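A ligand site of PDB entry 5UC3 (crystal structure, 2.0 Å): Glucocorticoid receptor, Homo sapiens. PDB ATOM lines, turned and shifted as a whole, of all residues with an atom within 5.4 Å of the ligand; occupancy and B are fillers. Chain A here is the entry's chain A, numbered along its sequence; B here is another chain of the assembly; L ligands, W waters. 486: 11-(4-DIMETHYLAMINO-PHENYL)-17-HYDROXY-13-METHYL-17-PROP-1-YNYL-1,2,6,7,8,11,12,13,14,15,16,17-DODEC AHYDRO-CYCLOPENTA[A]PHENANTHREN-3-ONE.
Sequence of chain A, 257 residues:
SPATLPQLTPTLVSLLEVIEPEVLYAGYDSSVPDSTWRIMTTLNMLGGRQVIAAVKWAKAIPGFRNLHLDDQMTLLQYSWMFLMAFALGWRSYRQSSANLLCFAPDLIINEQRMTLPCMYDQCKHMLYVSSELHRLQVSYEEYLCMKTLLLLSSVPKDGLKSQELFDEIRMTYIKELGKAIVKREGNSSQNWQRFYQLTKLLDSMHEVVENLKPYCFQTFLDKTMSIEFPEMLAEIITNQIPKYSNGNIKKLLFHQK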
ATOM      1  N   MET A  40      11.832 -11.950  37.384  1.00  0.00           N
ATOM      2  CA  MET A  40      12.864 -11.082  36.845  1.00  0.00           C
ATOM      3  C   MET A  40      14.223 -11.418  37.431  1.00  0.00           C
ATOM      4  O   MET A  40      15.231 -11.391  36.705  1.00  0.00           O
ATOM      5  CB  MET A  40      12.521  -9.609  37.115  1.00  0.00           C
ATOM      6  CG  MET A  40      11.290  -9.106  36.367  1.00  0.00           C
ATOM      7  SD  MET A  40      11.306  -9.488  34.606  1.00  0.00           S
ATOM      8  CE  MET A  40      12.829  -8.699  34.052  1.00  0.00           C
ATOM      9  N   LEU A  43      15.297 -14.500  35.581  1.00  0.00           N
ATOM     10  CA  LEU A  43      15.675 -14.179  34.204  1.00  0.00           C
ATOM     11  C   LEU A  43      17.016 -13.463  34.144  1.00  0.00           C
ATOM     12  O   LEU A  43      17.762 -13.630  33.168  1.00  0.00           O
ATOM     13  CB  LEU A  43      14.580 -13.344  33.555  1.00  0.00           C
ATOM     14  CG  LEU A  43      13.301 -14.151  33.313  1.00  0.00           C
ATOM     15  CD1 LEU A  43      12.250 -13.267  32.653  1.00  0.00           C
ATOM     16  CD2 LEU A  43      13.614 -15.409  32.488  1.00  0.00           C
ATOM     17  N   ASN A  44      17.361 -12.658  35.157  1.00  0.00           N
ATOM     18  CA  ASN A  44      18.659 -11.991  35.130  1.00  0.00           C
ATOM     19  C   ASN A  44      19.788 -13.006  35.246  1.00  0.00           C
ATOM     20  O   ASN A  44      20.784 -12.919  34.519  1.00  0.00           O
ATOM     21  CB  ASN A  44      18.759 -10.948  36.244  1.00  0.00           C
ATOM     22  CG  ASN A  44      18.302  -9.582  35.777  1.00  0.00           C
ATOM     23  OD1 ASN A  44      17.107  -9.334  35.635  1.00  0.00           O
ATOM     24  ND2 ASN A  44      19.249  -8.699  35.517  1.00  0.00           N
ATOM     25  N   LEU A  46      19.470 -16.248  34.513  1.00  0.00           N
ATOM     26  CA  LEU A  46      19.448 -17.012  33.266  1.00  0.00           C
ATOM     27  C   LEU A  46      20.090 -16.232  32.128  1.00  0.00           C
ATOM     28  O   LEU A  46      20.845 -16.793  31.327  1.00  0.00           O
ATOM     29  CB  LEU A  46      18.002 -17.414  32.924  1.00  0.00           C
ATOM     30  CG  LEU A  46      17.783 -18.206  31.627  1.00  0.00           C
ATOM     31  CD1 LEU A  46      18.468 -19.570  31.687  1.00  0.00           C
ATOM     32  CD2 LEU A  46      16.252 -18.349  31.342  1.00  0.00           C
ATOM     33  N   GLY A  47      19.827 -14.928  32.046  1.00  0.00           N
ATOM     34  CA  GLY A  47      20.441 -14.112  31.005  1.00  0.00           C
ATOM     35  C   GLY A  47      21.957 -14.157  31.049  1.00  0.00           C
ATOM     36  O   GLY A  47      22.620 -14.279  30.013  1.00  0.00           O
ATOM     37  N   GLY A  48      22.538 -14.059  32.253  1.00  0.00           N
ATOM     38  CA  GLY A  48      23.986 -14.137  32.368  1.00  0.00           C
ATOM     39  C   GLY A  48      24.537 -15.469  31.901  1.00  0.00           C
ATOM     40  O   GLY A  48      25.588 -15.524  31.254  1.00  0.00           O
ATOM     41  N   GLN A  50      23.160 -17.445  29.667  1.00  0.00           N
ATOM     42  CA  GLN A  50      23.043 -17.505  28.201  1.00  0.00           C
ATOM     43  C   GLN A  50      24.128 -16.669  27.513  1.00  0.00           C
ATOM     44  O   GLN A  50      24.590 -17.023  26.419  1.00  0.00           O
ATOM     45  CB  GLN A  50      21.638 -17.075  27.775  1.00  0.00           C
ATOM     46  CG  GLN A  50      20.587 -18.183  27.940  1.00  0.00           C
ATOM     47  CD  GLN A  50      19.215 -17.746  27.492  1.00  0.00           C
ATOM     48  OE1 GLN A  50      19.079 -16.727  26.805  1.00  0.00           O
ATOM     49  NE2 GLN A  50      18.189 -18.492  27.892  1.00  0.00           N
ATOM     50  N   VAL A  51      24.572 -15.582  28.130  1.00  0.00           N
ATOM     51  CA  VAL A  51      25.702 -14.838  27.556  1.00  0.00           C
ATOM     52  C   VAL A  51      26.953 -15.718  27.529  1.00  0.00           C
ATOM     53  O   VAL A  51      27.676 -15.757  26.516  1.00  0.00           O
ATOM     54  CB  VAL A  51      25.949 -13.524  28.328  1.00  0.00           C
ATOM     55  CG1 VAL A  51      27.266 -12.876  27.863  1.00  0.00           C
ATOM     56  CG2 VAL A  51      24.782 -12.578  28.115  1.00  0.00           C
ATOM     57  N   TRP A  80      24.711  -9.456  21.725  1.00  0.00           N
ATOM     58  CA  TRP A  80      24.211 -10.505  22.616  1.00  0.00           C
ATOM     59  C   TRP A  80      22.696 -10.470  22.811  1.00  0.00           C
ATOM     60  O   TRP A  80      22.047 -11.511  22.926  1.00  0.00           O
ATOM     61  CB  TRP A  80      24.917 -10.444  23.983  1.00  0.00           C
ATOM     62  CG  TRP A  80      24.601  -9.258  24.855  1.00  0.00           C
ATOM     63  CD1 TRP A  80      25.322  -8.101  24.977  1.00  0.00           C
ATOM     64  CD2 TRP A  80      23.459  -9.117  25.740  1.00  0.00           C
ATOM     65  NE1 TRP A  80      24.702  -7.248  25.881  1.00  0.00           N
ATOM     66  CE2 TRP A  80      23.571  -7.850  26.366  1.00  0.00           C
ATOM     67  CE3 TRP A  80      22.383  -9.934  26.062  1.00  0.00           C
ATOM     68  CZ2 TRP A  80      22.626  -7.396  27.289  1.00  0.00           C
ATOM     69  CZ3 TRP A  80      21.447  -9.478  26.979  1.00  0.00           C
ATOM     70  CH2 TRP A  80      21.575  -8.218  27.572  1.00  0.00           C
ATOM     71  N   MET A  81      22.106  -9.270  22.830  1.00  0.00           N
ATOM     72  CA  MET A  81      20.667  -9.179  23.029  1.00  0.00           C
ATOM     73  C   MET A  81      19.899  -9.587  21.782  1.00  0.00           C
ATOM     74  O   MET A  81      18.783 -10.107  21.889  1.00  0.00           O
ATOM     75  CB  MET A  81      20.291  -7.752  23.420  1.00  0.00           C
ATOM     76  CG  MET A  81      19.707  -7.675  24.782  1.00  0.00           C
ATOM     77  SD  MET A  81      18.012  -7.146  24.753  1.00  0.00           S
ATOM     78  CE  MET A  81      18.247  -5.410  24.836  1.00  0.00           C
ATOM     79  N   MET A  84      19.912 -13.382  21.981  1.00  0.00           N
ATOM     80  CA  MET A  84      19.078 -13.884  23.074  1.00  0.00           C
ATOM     81  C   MET A  84      17.595 -13.753  22.736  1.00  0.00           C
ATOM     82  O   MET A  84      16.822 -14.685  22.952  1.00  0.00           O
ATOM     83  CB  MET A  84      19.417 -13.110  24.345  1.00  0.00           C
ATOM     84  CG  MET A  84      19.133 -13.840  25.618  1.00  0.00           C
ATOM     85  SD  MET A  84      19.699 -12.890  27.045  1.00  0.00           S
ATOM     86  CE  MET A  84      21.445 -13.256  27.032  1.00  0.00           C
ATOM     87  N   ALA A  85      17.202 -12.599  22.196  1.00  0.00           N
ATOM     88  CA  ALA A  85      15.801 -12.371  21.865  1.00  0.00           C
ATOM     89  C   ALA A  85      15.357 -13.236  20.684  1.00  0.00           C
ATOM     90  O   ALA A  85      14.222 -13.720  20.644  1.00  0.00           O
ATOM     91  CB  ALA A  85      15.552 -10.893  21.561  1.00  0.00           C
ATOM     92  N   LEU A  88      15.114 -16.801  21.922  1.00  0.00           N
ATOM     93  CA  LEU A  88      13.888 -16.901  22.701  1.00  0.00           C
ATOM     94  C   LEU A  88      12.672 -17.006  21.782  1.00  0.00           C
ATOM     95  O   LEU A  88      11.745 -17.784  22.029  1.00  0.00           O
ATOM     96  CB  LEU A  88      13.749 -15.670  23.598  1.00  0.00           C
ATOM     97  CG  LEU A  88      12.427 -15.463  24.339  1.00  0.00           C
ATOM     98  CD1 LEU A  88      12.163 -16.517  25.402  1.00  0.00           C
ATOM     99  CD2 LEU A  88      12.391 -14.072  24.959  1.00  0.00           C
ATOM    100  N   ARG A  91      12.537 -20.583  20.512  1.00  0.00           N
ATOM    101  CA  ARG A  91      12.021 -21.553  21.475  1.00  0.00           C
ATOM    102  C   ARG A  91      10.525 -21.371  21.686  1.00  0.00           C
ATOM    103  O   ARG A  91       9.792 -22.357  21.872  1.00  0.00           O
ATOM    104  CB  ARG A  91      12.778 -21.462  22.817  1.00  0.00           C
ATOM    105  CG  ARG A  91      14.287 -21.834  22.681  1.00  0.00           C
ATOM    106  CD  ARG A  91      14.934 -22.039  24.047  1.00  0.00           C
ATOM    107  NE  ARG A  91      14.761 -20.866  24.913  1.00  0.00           N
ATOM    108  CZ  ARG A  91      15.530 -19.792  24.861  1.00  0.00           C
ATOM    109  NH1 ARG A  91      16.514 -19.719  23.965  1.00  0.00           N
ATOM    110  NH2 ARG A  91      15.310 -18.782  25.682  1.00  0.00           N
ATOM    111  N   PHE A 103      11.176 -18.883  27.973  1.00  0.00           N
ATOM    112  CA  PHE A 103      12.523 -18.530  28.443  1.00  0.00           C
ATOM    113  C   PHE A 103      13.348 -19.786  28.710  1.00  0.00           C
ATOM    114  O   PHE A 103      14.522 -19.867  28.333  1.00  0.00           O
ATOM    115  CB  PHE A 103      12.426 -17.647  29.691  1.00  0.00           C
ATOM    116  CG  PHE A 103      11.955 -16.252  29.396  1.00  0.00           C
ATOM    117  CD1 PHE A 103      12.837 -15.321  28.849  1.00  0.00           C
ATOM    118  CD2 PHE A 103      10.628 -15.885  29.584  1.00  0.00           C
ATOM    119  CE1 PHE A 103      12.425 -14.037  28.554  1.00  0.00           C
ATOM    120  CE2 PHE A 103      10.203 -14.594  29.273  1.00  0.00           C
ATOM    121  CZ  PHE A 103      11.119 -13.666  28.776  1.00  0.00           C
ATOM    122  N   MET A 119       5.055  -6.816  33.446  1.00  0.00           N
ATOM    123  CA  MET A 119       5.526  -7.881  32.567  1.00  0.00           C
ATOM    124  C   MET A 119       5.174  -7.650  31.105  1.00  0.00           C
ATOM    125  O   MET A 119       6.007  -7.861  30.211  1.00  0.00           O
ATOM    126  CB  MET A 119       4.976  -9.237  33.017  1.00  0.00           C
ATOM    127  CG  MET A 119       5.631  -9.828  34.248  1.00  0.00           C
ATOM    128  SD  MET A 119       7.372 -10.268  33.986  1.00  0.00           S
ATOM    129  CE  MET A 119       7.265 -11.233  32.497  1.00  0.00           C
ATOM    130  N   GLN A 122       7.318  -5.325  28.604  1.00  0.00           N
ATOM    131  CA  GLN A 122       8.541  -5.968  28.160  1.00  0.00           C
ATOM    132  C   GLN A 122       8.236  -7.040  27.132  1.00  0.00           C
ATOM    133  O   GLN A 122       8.848  -7.090  26.059  1.00  0.00           O
ATOM    134  CB  GLN A 122       9.250  -6.599  29.350  1.00  0.00           C
ATOM    135  CG  GLN A 122       9.523  -5.676  30.490  1.00  0.00           C
ATOM    136  CD  GLN A 122      10.314  -6.374  31.565  1.00  0.00           C
ATOM    137  OE1 GLN A 122      11.549  -6.289  31.605  1.00  0.00           O
ATOM    138  NE2 GLN A 122       9.616  -7.094  32.433  1.00  0.00           N
ATOM    139  N   CYS A 123       7.284  -7.914  27.442  1.00  0.00           N
ATOM    140  CA  CYS A 123       7.077  -9.128  26.667  1.00  0.00           C
ATOM    141  C   CYS A 123       6.544  -8.841  25.278  1.00  0.00           C
ATOM    142  O   CYS A 123       6.780  -9.635  24.359  1.00  0.00           O
ATOM    143  CB  CYS A 123       6.146 -10.057  27.435  1.00  0.00           C
ATOM    144  SG  CYS A 123       6.881 -10.682  28.978  1.00  0.00           S
ATOM    145  N   MET A 126       9.181  -8.916  22.708  1.00  0.00           N
ATOM    146  CA  MET A 126       9.729 -10.248  22.458  1.00  0.00           C
ATOM    147  C   MET A 126       8.726 -11.147  21.744  1.00  0.00           C
ATOM    148  O   MET A 126       9.140 -11.977  20.919  1.00  0.00           O
ATOM    149  CB  MET A 126      10.184 -10.856  23.784  1.00  0.00           C
ATOM    150  CG  MET A 126      11.416 -10.138  24.352  1.00  0.00           C
ATOM    151  SD  MET A 126      11.958 -10.749  25.956  1.00  0.00           S
ATOM    152  CE  MET A 126      10.822  -9.903  27.033  1.00  0.00           C
ATOM    153  N   LEU A 212      14.107  -3.175  24.107  1.00  0.00           N
ATOM    154  CA  LEU A 212      14.299  -4.008  25.282  1.00  0.00           C
ATOM    155  C   LEU A 212      15.418  -3.503  26.187  1.00  0.00           C
ATOM    156  O   LEU A 212      15.390  -3.737  27.402  1.00  0.00           O
ATOM    157  CB  LEU A 212      14.585  -5.462  24.856  1.00  0.00           C
ATOM    158  CG  LEU A 212      13.429  -6.218  24.173  1.00  0.00           C
ATOM    159  CD1 LEU A 212      13.917  -7.552  23.628  1.00  0.00           C
ATOM    160  CD2 LEU A 212      12.251  -6.430  25.138  1.00  0.00           C
ATOM    161  N   TYR A 215      14.662  -1.830  29.587  1.00  0.00           N
ATOM    162  CA  TYR A 215      14.185  -2.701  30.656  1.00  0.00           C
ATOM    163  C   TYR A 215      15.341  -3.483  31.284  1.00  0.00           C
ATOM    164  O   TYR A 215      15.350  -3.720  32.500  1.00  0.00           O
ATOM    165  CB  TYR A 215      13.121  -3.651  30.129  1.00  0.00           C
ATOM    166  CG  TYR A 215      11.858  -2.970  29.677  1.00  0.00           C
ATOM    167  CD1 TYR A 215      10.909  -2.527  30.592  1.00  0.00           C
ATOM    168  CD2 TYR A 215      11.598  -2.772  28.328  1.00  0.00           C
ATOM    169  CE1 TYR A 215       9.738  -1.899  30.171  1.00  0.00           C
ATOM    170  CE2 TYR A 215      10.432  -2.153  27.893  1.00  0.00           C
ATOM    171  CZ  TYR A 215       9.504  -1.716  28.820  1.00  0.00           C
ATOM    172  OH  TYR A 215       8.356  -1.104  28.375  1.00  0.00           O
ATOM    173  N   CYS A 216      16.304  -3.923  30.467  1.00  0.00           N
ATOM    174  CA  CYS A 216      17.513  -4.533  31.004  1.00  0.00           C
ATOM    175  C   CYS A 216      18.253  -3.572  31.925  1.00  0.00           C
ATOM    176  O   CYS A 216      18.663  -3.935  33.033  1.00  0.00           O
ATOM    177  CB  CYS A 216      18.422  -4.965  29.850  1.00  0.00           C
ATOM    178  SG  CYS A 216      19.917  -5.784  30.411  1.00  0.00           S
ATOM    179  N   THR A 219      16.208  -3.215  35.274  1.00  0.00           N
ATOM    180  CA  THR A 219      16.309  -4.322  36.231  1.00  0.00           C
ATOM    181  C   THR A 219      17.714  -4.415  36.829  1.00  0.00           C
ATOM    182  O   THR A 219      17.864  -4.768  38.005  1.00  0.00           O
ATOM    183  CB  THR A 219      15.862  -5.633  35.562  1.00  0.00           C
ATOM    184  OG1 THR A 219      16.058  -6.721  36.469  1.00  0.00           O
ATOM    185  CG2 THR A 219      16.658  -5.924  34.295  1.00  0.00           C
ATOM    186  N   PHE B 220      28.983  -2.090  33.385  1.00  0.00           N
ATOM    187  CA  PHE B 220      27.710  -2.522  32.818  1.00  0.00           C
ATOM    188  C   PHE B 220      27.282  -1.611  31.676  1.00  0.00           C
ATOM    189  O   PHE B 220      26.929  -2.092  30.579  1.00  0.00           O
ATOM    190  CB  PHE B 220      26.630  -2.551  33.913  1.00  0.00           C
ATOM    191  CG  PHE B 220      25.258  -2.828  33.389  1.00  0.00           C
ATOM    192  CD1 PHE B 220      24.845  -4.130  33.161  1.00  0.00           C
ATOM    193  CD2 PHE B 220      24.375  -1.787  33.138  1.00  0.00           C
ATOM    194  CE1 PHE B 220      23.565  -4.399  32.685  1.00  0.00           C
ATOM    195  CE2 PHE B 220      23.090  -2.036  32.662  1.00  0.00           C
ATOM    196  CZ  PHE B 220      22.686  -3.337  32.429  1.00  0.00           C
ATOM    197  N   THR B 224      28.146  -4.016  28.598  1.00  0.00           N
ATOM    198  CA  THR B 224      26.904  -4.755  28.432  1.00  0.00           C
ATOM    199  C   THR B 224      25.887  -3.977  27.608  1.00  0.00           C
ATOM    200  O   THR B 224      25.316  -4.519  26.658  1.00  0.00           O
ATOM    201  CB  THR B 224      26.313  -5.117  29.805  1.00  0.00           C
ATOM    202  OG1 THR B 224      27.192  -6.044  30.450  1.00  0.00           O
ATOM    203  CG2 THR B 224      24.926  -5.751  29.670  1.00  0.00           C
HETATM  204  O30 486 L   1      16.144 -16.718  27.523  1.00  0.00           O
HETATM  205  C2  486 L   1      16.412 -15.565  27.802  1.00  0.00           C
HETATM  206  C1  486 L   1      17.044 -15.183  29.128  1.00  0.00           C
HETATM  207  C3  486 L   1      16.077 -14.463  26.910  1.00  0.00           C
HETATM  208  C4  486 L   1      16.052 -13.172  27.298  1.00  0.00           C
HETATM  209  C7  486 L   1      15.634 -12.087  26.330  1.00  0.00           C
HETATM  210  C5  486 L   1      16.373 -12.768  28.675  1.00  0.00           C
HETATM  211  C6  486 L   1      16.480 -13.893  29.691  1.00  0.00           C
HETATM  212  C10 486 L   1      16.472 -11.474  29.031  1.00  0.00           C
HETATM  213  C14 486 L   1      16.652 -11.076  30.487  1.00  0.00           C
HETATM  214  C18 486 L   1      18.085 -10.646  30.798  1.00  0.00           C
HETATM  215  C22 486 L   1      18.399 -10.020  32.007  1.00  0.00           C
HETATM  216  C23 486 L   1      19.702  -9.615  32.297  1.00  0.00           C
HETATM  217  C24 486 L   1      20.762  -9.833  31.378  1.00  0.00           C
HETATM  218  N27 486 L   1      22.080  -9.436  31.634  1.00  0.00           N
HETATM  219  C29 486 L   1      22.310  -8.065  32.065  1.00  0.00           C
HETATM  220  C28 486 L   1      23.123 -10.023  30.785  1.00  0.00           C
HETATM  221  C25 486 L   1      20.432 -10.452  30.165  1.00  0.00           C
HETATM  222  C26 486 L   1      19.125 -10.848  29.889  1.00  0.00           C
HETATM  223  C13 486 L   1      15.525 -10.079  30.921  1.00  0.00           C
HETATM  224  C12 486 L   1      15.256  -8.985  29.869  1.00  0.00           C
HETATM  225  C19 486 L   1      16.374  -7.914  29.905  1.00  0.00           C
HETATM  226  C17 486 L   1      13.903  -8.216  29.986  1.00  0.00           C
HETATM  227  C31 486 L   1      12.773  -9.104  30.316  1.00  0.00           C
HETATM  228  C30 486 L   1      11.815  -9.786  30.581  1.00  0.00           C
HETATM  229  C32 486 L   1      10.632 -10.573  30.896  1.00  0.00           C
HETATM  230  O3  486 L   1      14.037  -7.228  31.026  1.00  0.00           O
HETATM  231  C16 486 L   1      13.732  -7.594  28.562  1.00  0.00           C
HETATM  232  C15 486 L   1      14.507  -8.509  27.580  1.00  0.00           C
HETATM  233  C11 486 L   1      15.066  -9.629  28.475  1.00  0.00           C
HETATM  234  C9  486 L   1      16.343 -10.333  28.040  1.00  0.00           C
HETATM  235  C8  486 L   1      16.366 -10.773  26.568  1.00  0.00           C
HETATM  236  O   HOH W   1      17.571 -16.916  24.571  1.00  0.00           O
HETATM  237  O   HOH W   2      22.716 -11.075  33.786  1.00  0.00           O
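The side-chain amide nitrogen (NE2) of Gln 50 is in hydrogen-bond range of an oxygen (O30) of the ligand, at 2.7 Å.
OE1 of Gln 122 is in hydrogen-bond range of O3 of the ligand.
An oxygen (O30) of the ligand lies within hydrogen-bond range of the guanidinium group of Arg 91 (2.9 Å).
The guanidinium group (NH2) of Arg 91 sits at hydrogen-bond distance from the backbone carbonyl oxygen (O) of Phe 103, 3.0 Å away.
The side-chain amide nitrogen (NE2) of Gln 122 lies within hydrogen-bond range of the side-chain sulfur (SD) of Met 40 (3.6 Å).
OG1 of Thr 219 is in hydrogen-bond range of OD1 of Asn 44.
NE1 of Trp 80 sits at hydrogen-bond distance from O of Thr 224 of chain B, 2.9 Å away.
The side-chain amide oxygen of Asn 44 lies close to the backbone carbonyl oxygen of Met 40, 3.0 Å away.
O of Met 119 sits at hydrogen-bond distance from SG of Cys 123, at 3.2 Å.
Met 40 touches the ligand.
CD1 of Leu 43 touches C32 of the ligand, 3.6 Å away.
Asn 44 touches the ligand (ND2 to C23, 3.4 Å).
Leu 46 touches the ligand (CD2 to C1, 3.9 Å).
Gly 47 touches the ligand.
Trp 80 touches the ligand (CZ3 to C25, 3.5 Å).
Met 84 touches the ligand (CG to C3, 3.4 Å).
O of Phe 103 touches O30 of the ligand, 3.6 Å away.
CE of Met 119 touches C32 of the ligand, 3.8 Å away.
Met 126 touches the ligand.
CD2 of Leu 212 touches C16 of the ligand, at 3.9 Å.
Tyr 215 touches the ligand (CB to O3, 3.8 Å).
Cys 216 touches the ligand.
CE1 of Phe 220 of chain B touches C29 of the ligand (3.9 Å).
The nearest printed residue that does not touch the ligand is Leu 88 (4.04 Å).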
